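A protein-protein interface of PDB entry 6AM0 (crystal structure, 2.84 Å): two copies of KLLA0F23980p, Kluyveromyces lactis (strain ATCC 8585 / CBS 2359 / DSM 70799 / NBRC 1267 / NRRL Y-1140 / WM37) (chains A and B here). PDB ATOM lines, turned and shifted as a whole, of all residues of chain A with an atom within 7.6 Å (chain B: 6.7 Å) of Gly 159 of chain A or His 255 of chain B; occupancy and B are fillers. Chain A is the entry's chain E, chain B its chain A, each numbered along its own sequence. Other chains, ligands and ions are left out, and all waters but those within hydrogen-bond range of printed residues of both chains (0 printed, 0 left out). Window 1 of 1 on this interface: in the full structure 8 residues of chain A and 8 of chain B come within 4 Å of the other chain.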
ATOM      1  N   VAL A 142       6.461  35.548 -18.000  1.00  0.00           N
ATOM      2  CA  VAL A 142       6.878  34.153 -18.075  1.00  0.00           C
ATOM      3  C   VAL A 142       7.393  33.680 -16.722  1.00  0.00           C
ATOM      4  O   VAL A 142       6.931  32.665 -16.193  1.00  0.00           O
ATOM      5  CB  VAL A 142       7.934  33.964 -19.177  1.00  0.00           C
ATOM      6  CG1 VAL A 142       8.300  32.496 -19.303  1.00  0.00           C
ATOM      7  CG2 VAL A 142       7.419  34.508 -20.498  1.00  0.00           C
ATOM      8  N   ILE A 146       5.859  30.639 -14.496  1.00  0.00           N
ATOM      9  CA  ILE A 146       6.642  29.500 -14.029  1.00  0.00           C
ATOM     10  C   ILE A 146       6.586  29.409 -12.514  1.00  0.00           C
ATOM     11  O   ILE A 146       6.532  28.312 -11.942  1.00  0.00           O
ATOM     12  CB  ILE A 146       8.094  29.600 -14.531  1.00  0.00           C
ATOM     13  CG1 ILE A 146       8.126  29.840 -16.039  1.00  0.00           C
ATOM     14  CG2 ILE A 146       8.853  28.328 -14.192  1.00  0.00           C
ATOM     15  CD1 ILE A 146       9.445  30.362 -16.545  1.00  0.00           C
ATOM     16  N   ASP A 156       8.147  22.658 -12.696  1.00  0.00           N
ATOM     17  CA  ASP A 156       8.933  23.745 -13.270  1.00  0.00           C
ATOM     18  C   ASP A 156       8.668  23.844 -14.770  1.00  0.00           C
ATOM     19  O   ASP A 156       8.988  22.919 -15.524  1.00  0.00           O
ATOM     20  CB  ASP A 156      10.418  23.513 -13.004  1.00  0.00           C
ATOM     21  CG  ASP A 156      11.249  24.767 -13.183  1.00  0.00           C
ATOM     22  OD1 ASP A 156      10.870  25.632 -13.996  1.00  0.00           O
ATOM     23  OD2 ASP A 156      12.286  24.887 -12.499  1.00  0.00           O
ATOM     24  N   LEU A 157       8.113  24.977 -15.207  1.00  0.00           N
ATOM     25  CA  LEU A 157       7.809  25.212 -16.614  1.00  0.00           C
ATOM     26  C   LEU A 157       8.818  26.134 -17.290  1.00  0.00           C
ATOM     27  O   LEU A 157       8.468  26.822 -18.255  1.00  0.00           O
ATOM     28  CB  LEU A 157       6.406  25.797 -16.775  1.00  0.00           C
ATOM     29  CG  LEU A 157       5.187  25.000 -16.321  1.00  0.00           C
ATOM     30  CD1 LEU A 157       3.958  25.509 -17.059  1.00  0.00           C
ATOM     31  CD2 LEU A 157       5.381  23.508 -16.542  1.00  0.00           C
ATOM     32  N   THR A 158      10.065  26.166 -16.813  1.00  0.00           N
ATOM     33  CA  THR A 158      11.021  27.133 -17.347  1.00  0.00           C
ATOM     34  C   THR A 158      11.379  26.848 -18.799  1.00  0.00           C
ATOM     35  O   THR A 158      11.801  27.758 -19.520  1.00  0.00           O
ATOM     36  CB  THR A 158      12.290  27.156 -16.501  1.00  0.00           C
ATOM     37  OG1 THR A 158      12.397  25.927 -15.782  1.00  0.00           O
ATOM     38  CG2 THR A 158      12.256  28.310 -15.516  1.00  0.00           C
ATOM     39  N   GLY A 159      11.224  25.608 -19.247  1.00  0.00           N
ATOM     40  CA  GLY A 159      11.576  25.282 -20.612  1.00  0.00           C
ATOM     41  C   GLY A 159      10.391  24.913 -21.479  1.00  0.00           C
ATOM     42  O   GLY A 159      10.561  24.244 -22.500  1.00  0.00           O
ATOM     43  N   PHE A 160       9.190  25.359 -21.110  1.00  0.00           N
ATOM     44  CA  PHE A 160       7.982  24.937 -21.807  1.00  0.00           C
ATOM     45  C   PHE A 160       7.094  26.092 -22.250  1.00  0.00           C
ATOM     46  O   PHE A 160       5.970  25.849 -22.700  1.00  0.00           O
ATOM     47  CB  PHE A 160       7.152  23.993 -20.928  1.00  0.00           C
ATOM     48  CG  PHE A 160       7.913  22.815 -20.400  1.00  0.00           C
ATOM     49  CD1 PHE A 160       8.646  22.915 -19.229  1.00  0.00           C
ATOM     50  CD2 PHE A 160       7.875  21.599 -21.058  1.00  0.00           C
ATOM     51  CE1 PHE A 160       9.340  21.831 -18.734  1.00  0.00           C
ATOM     52  CE2 PHE A 160       8.566  20.509 -20.567  1.00  0.00           C
ATOM     53  CZ  PHE A 160       9.300  20.625 -19.404  1.00  0.00           C
ATOM     54  N   ILE A 161       7.549  27.336 -22.137  1.00  0.00           N
ATOM     55  CA  ILE A 161       6.676  28.491 -22.291  1.00  0.00           C
ATOM     56  C   ILE A 161       7.174  29.354 -23.439  1.00  0.00           C
ATOM     57  O   ILE A 161       8.358  29.708 -23.490  1.00  0.00           O
ATOM     58  CB  ILE A 161       6.592  29.307 -20.988  1.00  0.00           C
ATOM     59  CG1 ILE A 161       6.062  28.422 -19.857  1.00  0.00           C
ATOM     60  CG2 ILE A 161       5.715  30.539 -21.180  1.00  0.00           C
ATOM     61  CD1 ILE A 161       5.716  29.164 -18.595  1.00  0.00           C
ATOM     62  N   ASP A 162       6.270  29.689 -24.355  1.00  0.00           N
ATOM     63  CA  ASP A 162       6.520  30.692 -25.380  1.00  0.00           C
ATOM     64  C   ASP A 162       5.844  31.992 -24.975  1.00  0.00           C
ATOM     65  O   ASP A 162       4.657  31.999 -24.628  1.00  0.00           O
ATOM     66  CB  ASP A 162       5.999  30.240 -26.746  1.00  0.00           C
ATOM     67  CG  ASP A 162       6.925  29.257 -27.431  1.00  0.00           C
ATOM     68  OD1 ASP A 162       7.613  28.492 -26.723  1.00  0.00           O
ATOM     69  OD2 ASP A 162       6.966  29.253 -28.680  1.00  0.00           O
ATOM     70  N   VAL A 181       0.948  25.766 -23.169  1.00  0.00           N
ATOM     71  CA  VAL A 181       2.092  24.866 -23.156  1.00  0.00           C
ATOM     72  C   VAL A 181       1.629  23.459 -23.506  1.00  0.00           C
ATOM     73  O   VAL A 181       0.462  23.097 -23.338  1.00  0.00           O
ATOM     74  CB  VAL A 181       2.826  24.866 -21.792  1.00  0.00           C
ATOM     75  CG1 VAL A 181       2.887  26.271 -21.217  1.00  0.00           C
ATOM     76  CG2 VAL A 181       2.175  23.895 -20.813  1.00  0.00           C
ATOM     77  N   LYS A 182       2.571  22.663 -24.006  1.00  0.00           N
ATOM     78  CA  LYS A 182       2.316  21.279 -24.365  1.00  0.00           C
ATOM     79  C   LYS A 182       3.553  20.455 -24.044  1.00  0.00           C
ATOM     80  O   LYS A 182       4.637  20.991 -23.792  1.00  0.00           O
ATOM     81  CB  LYS A 182       1.956  21.133 -25.847  1.00  0.00           C
ATOM     82  CG  LYS A 182       3.056  21.619 -26.770  1.00  0.00           C
ATOM     83  CD  LYS A 182       3.123  20.803 -28.045  1.00  0.00           C
ATOM     84  CE  LYS A 182       4.383  21.137 -28.825  1.00  0.00           C
ATOM     85  NZ  LYS A 182       4.404  20.490 -30.164  1.00  0.00           N
ATOM     86  N   GLY A 183       3.387  19.137 -24.068  1.00  0.00           N
ATOM     87  CA  GLY A 183       4.494  18.247 -23.802  1.00  0.00           C
ATOM     88  C   GLY A 183       4.781  18.008 -22.340  1.00  0.00           C
ATOM     89  O   GLY A 183       5.801  17.386 -22.021  1.00  0.00           O
ATOM     90  N   LEU B 250      17.170  18.117 -30.279  1.00  0.00           N
ATOM     91  CA  LEU B 250      16.040  18.983 -30.611  1.00  0.00           C
ATOM     92  C   LEU B 250      15.277  19.395 -29.356  1.00  0.00           C
ATOM     93  O   LEU B 250      14.981  20.583 -29.148  1.00  0.00           O
ATOM     94  CB  LEU B 250      15.124  18.265 -31.607  1.00  0.00           C
ATOM     95  CG  LEU B 250      14.008  19.028 -32.333  1.00  0.00           C
ATOM     96  CD1 LEU B 250      12.708  19.024 -31.537  1.00  0.00           C
ATOM     97  CD2 LEU B 250      14.443  20.452 -32.658  1.00  0.00           C
ATOM     98  N   TYR B 251      14.937  18.411 -28.514  1.00  0.00           N
ATOM     99  CA  TYR B 251      14.365  18.678 -27.196  1.00  0.00           C
ATOM    100  C   TYR B 251      15.138  19.781 -26.477  1.00  0.00           C
ATOM    101  O   TYR B 251      14.556  20.769 -26.001  1.00  0.00           O
ATOM    102  CB  TYR B 251      14.370  17.376 -26.388  1.00  0.00           C
ATOM    103  CG  TYR B 251      13.782  17.435 -24.995  1.00  0.00           C
ATOM    104  CD1 TYR B 251      12.420  17.256 -24.785  1.00  0.00           C
ATOM    105  CD2 TYR B 251      14.597  17.623 -23.884  1.00  0.00           C
ATOM    106  CE1 TYR B 251      11.883  17.290 -23.511  1.00  0.00           C
ATOM    107  CE2 TYR B 251      14.069  17.657 -22.607  1.00  0.00           C
ATOM    108  CZ  TYR B 251      12.713  17.491 -22.425  1.00  0.00           C
ATOM    109  OH  TYR B 251      12.182  17.529 -21.153  1.00  0.00           O
ATOM    110  N   ALA B 252      16.464  19.643 -26.427  1.00  0.00           N
ATOM    111  CA  ALA B 252      17.317  20.646 -25.805  1.00  0.00           C
ATOM    112  C   ALA B 252      17.102  22.021 -26.425  1.00  0.00           C
ATOM    113  O   ALA B 252      16.590  22.916 -25.752  1.00  0.00           O
ATOM    114  CB  ALA B 252      18.786  20.246 -25.908  1.00  0.00           C
ATOM    115  N   GLU B 253      17.462  22.195 -27.703  1.00  0.00           N
ATOM    116  CA  GLU B 253      17.442  23.532 -28.300  1.00  0.00           C
ATOM    117  C   GLU B 253      16.086  24.208 -28.146  1.00  0.00           C
ATOM    118  O   GLU B 253      16.013  25.422 -27.905  1.00  0.00           O
ATOM    119  CB  GLU B 253      17.835  23.473 -29.777  1.00  0.00           C
ATOM    120  CG  GLU B 253      17.225  22.332 -30.564  1.00  0.00           C
ATOM    121  CD  GLU B 253      17.922  22.113 -31.895  1.00  0.00           C
ATOM    122  OE1 GLU B 253      18.072  23.092 -32.657  1.00  0.00           O
ATOM    123  OE2 GLU B 253      18.334  20.966 -32.173  1.00  0.00           O
ATOM    124  N   GLU B 254      15.000  23.442 -28.268  1.00  0.00           N
ATOM    125  CA  GLU B 254      13.688  24.045 -28.060  1.00  0.00           C
ATOM    126  C   GLU B 254      13.525  24.515 -26.618  1.00  0.00           C
ATOM    127  O   GLU B 254      13.056  25.635 -26.368  1.00  0.00           O
ATOM    128  CB  GLU B 254      12.586  23.058 -28.448  1.00  0.00           C
ATOM    129  CG  GLU B 254      11.225  23.709 -28.625  1.00  0.00           C
ATOM    130  CD  GLU B 254      10.321  22.928 -29.559  1.00  0.00           C
ATOM    131  OE1 GLU B 254       9.117  23.257 -29.633  1.00  0.00           O
ATOM    132  OE2 GLU B 254      10.815  21.989 -30.220  1.00  0.00           O
ATOM    133  N   HIS B 255      13.943  23.687 -25.654  1.00  0.00           N
ATOM    134  CA  HIS B 255      13.810  24.078 -24.253  1.00  0.00           C
ATOM    135  C   HIS B 255      14.676  25.288 -23.910  1.00  0.00           C
ATOM    136  O   HIS B 255      14.237  26.177 -23.172  1.00  0.00           O
ATOM    137  CB  HIS B 255      14.147  22.899 -23.346  1.00  0.00           C
ATOM    138  CG  HIS B 255      12.993  21.982 -23.107  1.00  0.00           C
ATOM    139  ND1 HIS B 255      11.682  22.387 -23.240  1.00  0.00           N
ATOM    140  CD2 HIS B 255      12.948  20.678 -22.748  1.00  0.00           C
ATOM    141  CE1 HIS B 255      10.880  21.373 -22.971  1.00  0.00           C
ATOM    142  NE2 HIS B 255      11.623  20.324 -22.669  1.00  0.00           N
ATOM    143  N   LEU B 256      15.911  25.339 -24.419  1.00  0.00           N
ATOM    144  CA  LEU B 256      16.759  26.502 -24.170  1.00  0.00           C
ATOM    145  C   LEU B 256      16.146  27.757 -24.770  1.00  0.00           C
ATOM    146  O   LEU B 256      16.114  28.814 -24.129  1.00  0.00           O
ATOM    147  CB  LEU B 256      18.165  26.277 -24.730  1.00  0.00           C
ATOM    148  CG  LEU B 256      19.177  25.505 -23.883  1.00  0.00           C
ATOM    149  CD1 LEU B 256      19.000  24.013 -24.063  1.00  0.00           C
ATOM    150  CD2 LEU B 256      20.595  25.922 -24.241  1.00  0.00           C
ATOM    151  N   LYS B 257      15.644  27.664 -26.006  1.00  0.00           N
ATOM    152  CA  LYS B 257      14.958  28.813 -26.583  1.00  0.00           C
ATOM    153  C   LYS B 257      13.669  29.149 -25.846  1.00  0.00           C
ATOM    154  O   LYS B 257      13.122  30.239 -26.056  1.00  0.00           O
ATOM    155  CB  LYS B 257      14.669  28.578 -28.067  1.00  0.00           C
ATOM    156  CG  LYS B 257      15.663  29.264 -28.991  1.00  0.00           C
ATOM    157  CD  LYS B 257      15.193  29.237 -30.436  1.00  0.00           C
ATOM    158  CE  LYS B 257      16.145  30.010 -31.337  1.00  0.00           C
ATOM    159  NZ  LYS B 257      15.711  30.009 -32.763  1.00  0.00           N
ATOM    160  N   SER B 258      13.172  28.248 -24.994  1.00  0.00           N
ATOM    161  CA  SER B 258      12.079  28.602 -24.094  1.00  0.00           C
ATOM    162  C   SER B 258      12.585  29.330 -22.853  1.00  0.00           C
ATOM    163  O   SER B 258      11.965  30.303 -22.408  1.00  0.00           O
ATOM    164  CB  SER B 258      11.301  27.352 -23.687  1.00  0.00           C
ATOM    165  OG  SER B 258      10.378  27.646 -22.653  1.00  0.00           O
ATOM    166  N   ILE B 259      13.697  28.866 -22.275  1.00  0.00           N
ATOM    167  CA  ILE B 259      14.251  29.511 -21.087  1.00  0.00           C
ATOM    168  C   ILE B 259      14.615  30.957 -21.394  1.00  0.00           C
ATOM    169  O   ILE B 259      14.292  31.876 -20.633  1.00  0.00           O
ATOM    170  CB  ILE B 259      15.463  28.720 -20.562  1.00  0.00           C
ATOM    171  CG1 ILE B 259      15.008  27.371 -20.004  1.00  0.00           C
ATOM    172  CG2 ILE B 259      16.203  29.515 -19.501  1.00  0.00           C
ATOM    173  CD1 ILE B 259      16.124  26.546 -19.414  1.00  0.00           C
ATOM    174  N   LEU B 260      15.280  31.180 -22.520  1.00  0.00           N
ATOM    175  CA  LEU B 260      15.580  32.525 -22.978  1.00  0.00           C
ATOM    176  C   LEU B 260      14.417  33.019 -23.836  1.00  0.00           C
ATOM    177  O   LEU B 260      13.359  32.387 -23.909  1.00  0.00           O
ATOM    178  CB  LEU B 260      16.909  32.550 -23.732  1.00  0.00           C
ATOM    179  CG  LEU B 260      18.201  32.243 -22.965  1.00  0.00           C
ATOM    180  CD1 LEU B 260      18.346  30.765 -22.626  1.00  0.00           C
ATOM    181  CD2 LEU B 260      19.400  32.713 -23.763  1.00  0.00           C
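Of the printed residues of chain B, Thr 158 of chain A touches Ser 258 (3.4 Å) and Ile 259 (3.3 Å).
Gly 159 of chain A touches two residues of chain B.
Of the printed residues of chain B, Phe 160 of chain A touches His 255 (3.4 Å) and Ser 258 (3.0 Å).
Of the printed residues of chain A, His 255 of chain B touches Gly 159 (2.3 Å) and Phe 160 (3.4 Å).
Of the printed residues of chain A, Ile 259 of chain B touches Thr 158.
The nearest residue of chain B that does not touch Gly 159 of chain A is Ile 259 of chain B (4.1 Å).
The nearest residue of chain A that does not touch His 255 of chain B is Thr 158 of chain A (4.7 Å).
The nearest printed residue of chain A that does not touch Ile 259 of chain B is Gly 159 of chain A (4.1 Å).
The side-chain hydroxyl (OH) of Tyr 251 of chain B sits close to a ring nitrogen (NE2) of His 255 of chain B.
The side-chain carboxylate (OD1) of Asp 156 of chain A sits at hydrogen-bond distance from the backbone NH (N) of Thr 158 of chain A (3.0 Å).
Of the 12 printed residues of chain A, 4 touch a printed residue of chain B.
Among the printed residues, 7 pairs touch across the chains.
The side-chain hydroxyl (OG) of Ser 258 of chain B lies within hydrogen-bond range of the backbone carbonyl oxygen (O) of Thr 158 of chain A, at 3.4 Å.
OG of Ser 258 of chain B sits close to O of Gly 159 of chain A.
The backbone NH (N) of Phe 160 of chain A is in hydrogen-bond range of the side-chain hydroxyl (OG) of Ser 258 of chain B (3.0 Å).
The side-chain hydroxyl (OG) of Ser 258 of chain B is in hydrogen-bond range of the backbone NH (N) of Ile 161 of chain A (2.9 Å).
O of Gly 159 of chain A lies close to ND1 of His 255 of chain B (2.3 Å).
Ile 259 of chain B touches Thr 158 of chain A (CG1 to O, 3.3 Å).
His 255 of chain B touches Phe 160 of chain A (CE1 to CE2, 3.4 Å).
No position is printed for both chains.
Of the 7 pairs that touch across the chains among the printed residues, none has its exchanged pair printed and touching as well.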
